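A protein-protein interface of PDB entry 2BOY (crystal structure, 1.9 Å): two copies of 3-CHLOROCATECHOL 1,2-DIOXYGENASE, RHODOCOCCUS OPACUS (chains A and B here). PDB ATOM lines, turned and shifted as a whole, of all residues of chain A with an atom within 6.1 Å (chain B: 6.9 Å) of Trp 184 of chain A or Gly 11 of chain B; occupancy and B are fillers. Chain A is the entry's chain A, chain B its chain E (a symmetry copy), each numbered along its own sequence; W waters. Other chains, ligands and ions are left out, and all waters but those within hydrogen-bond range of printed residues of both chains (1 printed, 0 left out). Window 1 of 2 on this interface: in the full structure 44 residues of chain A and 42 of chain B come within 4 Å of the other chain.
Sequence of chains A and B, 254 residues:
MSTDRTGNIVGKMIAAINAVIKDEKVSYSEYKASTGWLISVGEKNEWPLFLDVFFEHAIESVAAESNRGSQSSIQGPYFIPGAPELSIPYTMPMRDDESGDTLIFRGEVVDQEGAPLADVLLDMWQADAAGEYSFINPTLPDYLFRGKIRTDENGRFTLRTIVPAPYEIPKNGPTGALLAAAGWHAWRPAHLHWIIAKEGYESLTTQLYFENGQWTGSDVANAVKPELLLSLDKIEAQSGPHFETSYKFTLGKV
The backbone carbonyl oxygen of Ala 181 of chain A lies within hydrogen-bond range of the side-chain hydroxyl of Thr 3 of chain B, 3.4 Å away. The backbone NH (N) of Gly 183 of chain A lies within hydrogen-bond range of the side-chain hydroxyl (OG1) of Thr 3 of chain B, at 3.3 Å.
The backbone carbonyl oxygen of Leu 179 of chain A is in hydrogen-bond range of the backbone NH of Trp 184 of chain A, at 3.0 Å. The backbone carbonyl oxygen (O) of Ala 182 of chain A sits close to the indole nitrogen (NE1) of Trp 184 of chain A, at 3.3 Å.
Phe 54 of chain A touches Ile 14 of chain B. O of Ala 180 of chain A touches OG1 of Thr 3 of chain B, 3.9 Å away. O of Ala 181 of chain A touches CB of Thr 6 of chain B, 3.7 Å away. Thr 3 of chain B touches Ala 182 of chain A (O to O, 3.5 Å). Ala 182 of chain A touches Gly 7 of chain B (CB to CA, 3.6 Å). Gly 7 of chain B touches Trp 184 of chain A (O to CZ2, 3.3 Å). CH2 of Trp 184 of chain A touches C of Val 10 of chain B (3.9997 Å). Gly 11 of chain B touches Trp 184 of chain A.
Leu 178 of chain A touches none of the printed residues of chain B. Printed residues of chain B within 4 Å of Ala 181 of chain A: Thr 3 (3.4 Å) and Thr 6 (3.7 Å). Of chain B, only Thr 3 comes within 4 Å of Gly 183 of chain A. Printed residues of chain B within 4 Å of Trp 184 of chain A: Gly 7, Val 10 and Gly 11. Of the printed residues of chain A, Thr 3 of chain B touches Ala 180, Ala 181, Ala 182 and Gly 183. Printed residues of chain A within 4 Å of Gly 7 of chain B: Ala 182 and Trp 184. Of chain A, only Trp 184 (3.5 Å) comes within 4 Å of Gly 11 of chain B. Of the printed residues of chain A, Ile 14 of chain B touches Phe 54 (3.5 Å). The nearest printed residue of chain A that does not touch Gly 11 of chain B is Ala 182 of chain A (6.2 Å).
Printed residues of chain A that touch a printed residue of chain B: Phe 54, Ala 180, Ala 181, Ala 182, Gly 183 and Trp 184. Hydrophobic or aromatic side chains of chain A that line the printed part of chain B: Phe 54, Ala 182 and Trp 184. Along chain A the printed residues that touch a printed residue of chain B span positions 54 to 184. Of the 13 printed residues of chain B, 6 touch a printed residue of chain A. Hydrophobic or aromatic side chains of chain B within 4 Å of the printed part of chain A: Ile 14. Among the printed residues, 10 pairs touch across the chains. Among the printed residues, no Asp or Glu carboxylate lies within 4 Å of a Lys or Arg side-chain nitrogen of the other chain.
No position is printed for both chains.
Water W1 bridges the backbone carbonyl oxygen of Ala 181 of chain A (2.9 Å) and the side-chain hydroxyl of Thr 6 of chain B (3.0 Å).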
ATOM      1  N   PHE A  54       2.123  16.816  22.207  1.00  0.00           N
ATOM      2  CA  PHE A  54       1.161  17.850  21.833  1.00  0.00           C
ATOM      3  C   PHE A  54       0.691  17.855  20.391  1.00  0.00           C
ATOM      4  O   PHE A  54      -0.397  18.374  20.093  1.00  0.00           O
ATOM      5  CB  PHE A  54       1.746  19.229  22.195  1.00  0.00           C
ATOM      6  CG  PHE A  54       1.802  19.460  23.686  1.00  0.00           C
ATOM      7  CD1 PHE A  54       0.629  19.612  24.398  1.00  0.00           C
ATOM      8  CD2 PHE A  54       3.012  19.475  24.363  1.00  0.00           C
ATOM      9  CE1 PHE A  54       0.673  19.828  25.790  1.00  0.00           C
ATOM     10  CE2 PHE A  54       3.058  19.655  25.739  1.00  0.00           C
ATOM     11  CZ  PHE A  54       1.885  19.851  26.431  1.00  0.00           C
ATOM     12  N   LEU A 178       6.366  22.392  31.494  1.00  0.00           N
ATOM     13  CA  LEU A 178       5.285  23.159  30.882  1.00  0.00           C
ATOM     14  C   LEU A 178       3.883  22.663  31.328  1.00  0.00           C
ATOM     15  O   LEU A 178       2.986  23.468  31.621  1.00  0.00           O
ATOM     16  CB  LEU A 178       5.382  23.074  29.350  1.00  0.00           C
ATOM     17  CG  LEU A 178       4.143  23.536  28.579  1.00  0.00           C
ATOM     18  CD1 LEU A 178       3.921  25.050  28.751  1.00  0.00           C
ATOM     19  CD2 LEU A 178       4.346  23.189  27.123  1.00  0.00           C
ATOM     20  N   LEU A 179       3.686  21.341  31.327  1.00  0.00           N
ATOM     21  CA  LEU A 179       2.379  20.770  31.697  1.00  0.00           C
ATOM     22  C   LEU A 179       2.057  21.248  33.120  1.00  0.00           C
ATOM     23  O   LEU A 179       0.932  21.690  33.430  1.00  0.00           O
ATOM     24  CB  LEU A 179       2.450  19.242  31.695  1.00  0.00           C
ATOM     25  CG  LEU A 179       2.408  18.638  30.291  1.00  0.00           C
ATOM     26  CD1 LEU A 179       2.985  17.236  30.258  1.00  0.00           C
ATOM     27  CD2 LEU A 179       0.994  18.708  29.690  1.00  0.00           C
ATOM     28  N   ALA A 180       3.065  21.163  33.974  1.00  0.00           N
ATOM     29  CA  ALA A 180       2.895  21.575  35.366  1.00  0.00           C
ATOM     30  C   ALA A 180       2.534  23.072  35.470  1.00  0.00           C
ATOM     31  O   ALA A 180       1.532  23.473  36.138  1.00  0.00           O
ATOM     32  CB  ALA A 180       4.154  21.215  36.184  1.00  0.00           C
ATOM     33  N   ALA A 181       3.269  23.900  34.725  1.00  0.00           N
ATOM     34  CA  ALA A 181       3.027  25.348  34.732  1.00  0.00           C
ATOM     35  C   ALA A 181       1.687  25.756  34.134  1.00  0.00           C
ATOM     36  O   ALA A 181       1.116  26.772  34.549  1.00  0.00           O
ATOM     37  CB  ALA A 181       4.192  26.103  34.043  1.00  0.00           C
ATOM     38  N   ALA A 182       1.163  24.985  33.171  1.00  0.00           N
ATOM     39  CA  ALA A 182      -0.164  25.295  32.579  1.00  0.00           C
ATOM     40  C   ALA A 182      -1.367  24.693  33.335  1.00  0.00           C
ATOM     41  O   ALA A 182      -2.503  24.813  32.873  1.00  0.00           O
ATOM     42  CB  ALA A 182      -0.237  24.863  31.089  1.00  0.00           C
ATOM     43  N   GLY A 183      -1.116  24.040  34.467  1.00  0.00           N
ATOM     44  CA  GLY A 183      -2.141  23.352  35.235  1.00  0.00           C
ATOM     45  C   GLY A 183      -2.770  22.127  34.563  1.00  0.00           C
ATOM     46  O   GLY A 183      -3.920  21.793  34.857  1.00  0.00           O
ATOM     47  N   TRP A 184      -2.045  21.475  33.653  1.00  0.00           N
ATOM     48  CA  TRP A 184      -2.593  20.349  32.887  1.00  0.00           C
ATOM     49  C   TRP A 184      -2.086  19.036  33.436  1.00  0.00           C
ATOM     50  O   TRP A 184      -0.916  18.924  33.770  1.00  0.00           O
ATOM     51  CB  TRP A 184      -2.153  20.460  31.426  1.00  0.00           C
ATOM     52  CG  TRP A 184      -2.662  21.685  30.713  1.00  0.00           C
ATOM     53  CD1 TRP A 184      -3.721  22.482  31.060  1.00  0.00           C
ATOM     54  CD2 TRP A 184      -2.128  22.228  29.516  1.00  0.00           C
ATOM     55  NE1 TRP A 184      -3.865  23.501  30.151  1.00  0.00           N
ATOM     56  CE2 TRP A 184      -2.899  23.363  29.186  1.00  0.00           C
ATOM     57  CE3 TRP A 184      -1.034  21.887  28.698  1.00  0.00           C
ATOM     58  CZ2 TRP A 184      -2.622  24.163  28.073  1.00  0.00           C
ATOM     59  CZ3 TRP A 184      -0.751  22.690  27.574  1.00  0.00           C
ATOM     60  CH2 TRP A 184      -1.553  23.803  27.268  1.00  0.00           C
ATOM     61  N   HIS A 185      -2.958  18.041  33.559  1.00  0.00           N
ATOM     62  CA  HIS A 185      -2.526  16.707  33.942  1.00  0.00           C
ATOM     63  C   HIS A 185      -1.496  16.200  32.944  1.00  0.00           C
ATOM     64  O   HIS A 185      -1.627  16.454  31.730  1.00  0.00           O
ATOM     65  CB  HIS A 185      -3.726  15.763  33.891  1.00  0.00           C
ATOM     66  CG  HIS A 185      -4.688  15.971  35.016  1.00  0.00           C
ATOM     67  ND1 HIS A 185      -6.029  16.266  34.817  1.00  0.00           N
ATOM     68  CD2 HIS A 185      -4.500  15.920  36.355  1.00  0.00           C
ATOM     69  CE1 HIS A 185      -6.625  16.355  36.002  1.00  0.00           C
ATOM     70  NE2 HIS A 185      -5.716  16.165  36.943  1.00  0.00           N
ATOM     71  N   ALA A 186      -0.492  15.487  33.461  1.00  0.00           N
ATOM     72  CA  ALA A 186       0.581  14.980  32.626  1.00  0.00           C
ATOM     73  C   ALA A 186       0.458  13.484  32.333  1.00  0.00           C
ATOM     74  O   ALA A 186       1.456  12.848  32.017  1.00  0.00           O
ATOM     75  CB  ALA A 186       1.913  15.275  33.314  1.00  0.00           C
ATOM     76  N   VAL A 220      -3.089  12.987  28.218  1.00  0.00           N
ATOM     77  CA  VAL A 220      -2.256  14.185  27.927  1.00  0.00           C
ATOM     78  C   VAL A 220      -1.866  14.282  26.401  1.00  0.00           C
ATOM     79  O   VAL A 220      -1.748  15.384  25.819  1.00  0.00           O
ATOM     80  CB  VAL A 220      -0.973  14.226  28.817  1.00  0.00           C
ATOM     81  CG1 VAL A 220      -0.071  13.123  28.438  1.00  0.00           C
ATOM     82  CG2 VAL A 220      -0.246  15.606  28.680  1.00  0.00           C
ATOM     83  N   THR B   3      -1.079  29.686  36.505  1.00  0.00           N
ATOM     84  CA  THR B   3      -1.491  28.386  35.961  1.00  0.00           C
ATOM     85  C   THR B   3      -2.675  28.610  34.987  1.00  0.00           C
ATOM     86  O   THR B   3      -2.638  28.181  33.837  1.00  0.00           O
ATOM     87  CB  THR B   3      -1.777  27.424  37.166  1.00  0.00           C
ATOM     88  OG1 THR B   3      -1.144  26.154  36.963  1.00  0.00           O
ATOM     89  CG2 THR B   3      -3.203  27.118  37.358  1.00  0.00           C
ATOM     90  N   ARG B   5      -3.473  31.455  33.410  1.00  0.00           N
ATOM     91  CA  ARG B   5      -3.035  32.269  32.270  1.00  0.00           C
ATOM     92  C   ARG B   5      -2.112  31.498  31.316  1.00  0.00           C
ATOM     93  O   ARG B   5      -2.269  31.567  30.104  1.00  0.00           O
ATOM     94  CB  ARG B   5      -2.353  33.551  32.770  1.00  0.00           C
ATOM     95  CG  ARG B   5      -1.656  34.342  31.665  1.00  0.00           C
ATOM     96  CD  ARG B   5      -1.163  35.736  32.078  1.00  0.00           C
ATOM     97  NE  ARG B   5      -0.457  36.384  30.965  1.00  0.00           N
ATOM     98  CZ  ARG B   5      -1.053  37.072  30.000  1.00  0.00           C
ATOM     99  NH1 ARG B   5      -2.374  37.218  30.006  1.00  0.00           N
ATOM    100  NH2 ARG B   5      -0.339  37.638  29.020  1.00  0.00           N
ATOM    101  N   THR B   6      -1.133  30.803  31.867  1.00  0.00           N
ATOM    102  CA  THR B   6      -0.210  29.967  31.066  1.00  0.00           C
ATOM    103  C   THR B   6      -0.956  28.902  30.234  1.00  0.00           C
ATOM    104  O   THR B   6      -0.728  28.784  29.014  1.00  0.00           O
ATOM    105  CB  THR B   6       0.795  29.340  31.974  1.00  0.00           C
ATOM    106  OG1 THR B   6       1.522  30.396  32.613  1.00  0.00           O
ATOM    107  CG2 THR B   6       1.867  28.510  31.187  1.00  0.00           C
ATOM    108  N   GLY B   7      -1.879  28.196  30.880  1.00  0.00           N
ATOM    109  CA  GLY B   7      -2.752  27.267  30.184  1.00  0.00           C
ATOM    110  C   GLY B   7      -3.517  27.902  29.063  1.00  0.00           C
ATOM    111  O   GLY B   7      -3.591  27.359  27.957  1.00  0.00           O
ATOM    112  N   ASN B   8      -4.105  29.067  29.338  1.00  0.00           N
ATOM    113  CA  ASN B   8      -4.887  29.765  28.338  1.00  0.00           C
ATOM    114  C   ASN B   8      -4.060  30.091  27.106  1.00  0.00           C
ATOM    115  O   ASN B   8      -4.466  29.777  25.997  1.00  0.00           O
ATOM    116  CB  ASN B   8      -5.431  31.087  28.917  1.00  0.00           C
ATOM    117  CG  ASN B   8      -6.725  30.921  29.686  1.00  0.00           C
ATOM    118  OD1 ASN B   8      -7.305  29.841  29.743  1.00  0.00           O
ATOM    119  ND2 ASN B   8      -7.168  31.999  30.303  1.00  0.00           N
ATOM    120  N   ILE B   9      -2.914  30.741  27.309  1.00  0.00           N
ATOM    121  CA  ILE B   9      -2.058  31.183  26.215  1.00  0.00           C
ATOM    122  C   ILE B   9      -1.459  29.980  25.477  1.00  0.00           C
ATOM    123  O   ILE B   9      -1.574  29.882  24.269  1.00  0.00           O
ATOM    124  CB  ILE B   9      -0.934  32.085  26.758  1.00  0.00           C
ATOM    125  CG1 ILE B   9      -1.499  33.409  27.330  1.00  0.00           C
ATOM    126  CG2 ILE B   9       0.104  32.364  25.668  1.00  0.00           C
ATOM    127  CD1 ILE B   9      -0.471  34.151  28.185  1.00  0.00           C
ATOM    128  N   VAL B  10      -0.818  29.076  26.209  1.00  0.00           N
ATOM    129  CA  VAL B  10      -0.201  27.918  25.562  1.00  0.00           C
ATOM    130  C   VAL B  10      -1.248  27.009  24.896  1.00  0.00           C
ATOM    131  O   VAL B  10      -1.063  26.559  23.766  1.00  0.00           O
ATOM    132  CB  VAL B  10       0.727  27.151  26.525  1.00  0.00           C
ATOM    133  CG1 VAL B  10       1.443  26.028  25.754  1.00  0.00           C
ATOM    134  CG2 VAL B  10       1.768  28.138  27.154  1.00  0.00           C
ATOM    135  N   GLY B  11      -2.357  26.756  25.575  1.00  0.00           N
ATOM    136  CA  GLY B  11      -3.415  25.960  24.976  1.00  0.00           C
ATOM    137  C   GLY B  11      -3.922  26.512  23.643  1.00  0.00           C
ATOM    138  O   GLY B  11      -4.159  25.744  22.705  1.00  0.00           O
ATOM    139  N   LYS B  12      -4.121  27.830  23.569  1.00  0.00           N
ATOM    140  CA  LYS B  12      -4.613  28.437  22.317  1.00  0.00           C
ATOM    141  C   LYS B  12      -3.581  28.272  21.211  1.00  0.00           C
ATOM    142  O   LYS B  12      -3.929  28.053  20.042  1.00  0.00           O
ATOM    143  CB  LYS B  12      -4.882  29.941  22.528  1.00  0.00           C
ATOM    144  CG  LYS B  12      -6.247  30.251  23.151  1.00  0.00           C
ATOM    145  CD  LYS B  12      -6.291  31.712  23.614  1.00  0.00           C
ATOM    146  CE  LYS B  12      -7.559  32.007  24.397  1.00  0.00           C
ATOM    147  NZ  LYS B  12      -7.863  33.496  24.381  1.00  0.00           N
ATOM    148  N   MET B  13      -2.297  28.384  21.568  1.00  0.00           N
ATOM    149  CA  MET B  13      -1.236  28.268  20.567  1.00  0.00           C
ATOM    150  C   MET B  13      -1.105  26.841  20.027  1.00  0.00           C
ATOM    151  O   MET B  13      -0.997  26.620  18.817  1.00  0.00           O
ATOM    152  CB  MET B  13       0.119  28.746  21.139  1.00  0.00           C
ATOM    153  CG  MET B  13       0.169  30.247  21.421  1.00  0.00           C
ATOM    154  SD  MET B  13       1.782  30.730  22.017  1.00  0.00           S
ATOM    155  CE  MET B  13       1.559  32.581  22.143  1.00  0.00           C
ATOM    156  N   ILE B  14      -1.101  25.882  20.936  1.00  0.00           N
ATOM    157  CA  ILE B  14      -1.044  24.466  20.544  1.00  0.00           C
ATOM    158  C   ILE B  14      -2.279  24.144  19.706  1.00  0.00           C
ATOM    159  O   ILE B  14      -2.170  23.530  18.665  1.00  0.00           O
ATOM    160  CB  ILE B  14      -0.945  23.567  21.812  1.00  0.00           C
ATOM    161  CG1 ILE B  14       0.435  23.762  22.464  1.00  0.00           C
ATOM    162  CG2 ILE B  14      -1.166  22.084  21.435  1.00  0.00           C
ATOM    163  CD1 ILE B  14       0.607  23.040  23.824  1.00  0.00           C
ATOM    164  N   ALA B  15      -3.455  24.598  20.146  1.00  0.00           N
ATOM    165  CA  ALA B  15      -4.676  24.328  19.362  1.00  0.00           C
ATOM    166  C   ALA B  15      -4.622  24.904  17.940  1.00  0.00           C
ATOM    167  O   ALA B  15      -5.083  24.259  16.981  1.00  0.00           O
ATOM    168  CB  ALA B  15      -5.953  24.780  20.128  1.00  0.00           C
ATOM    169  N   ALA B  16      -4.084  26.115  17.806  1.00  0.00           N
ATOM    170  CA  ALA B  16      -4.015  26.765  16.492  1.00  0.00           C
ATOM    171  C   ALA B  16      -3.046  26.008  15.586  1.00  0.00           C
ATOM    172  O   ALA B  16      -3.295  25.869  14.395  1.00  0.00           O
ATOM    173  CB  ALA B  16      -3.562  28.244  16.625  1.00  0.00           C
HETATM  174  O   HOH W   1       2.496  29.233  35.229  1.00  0.00           O
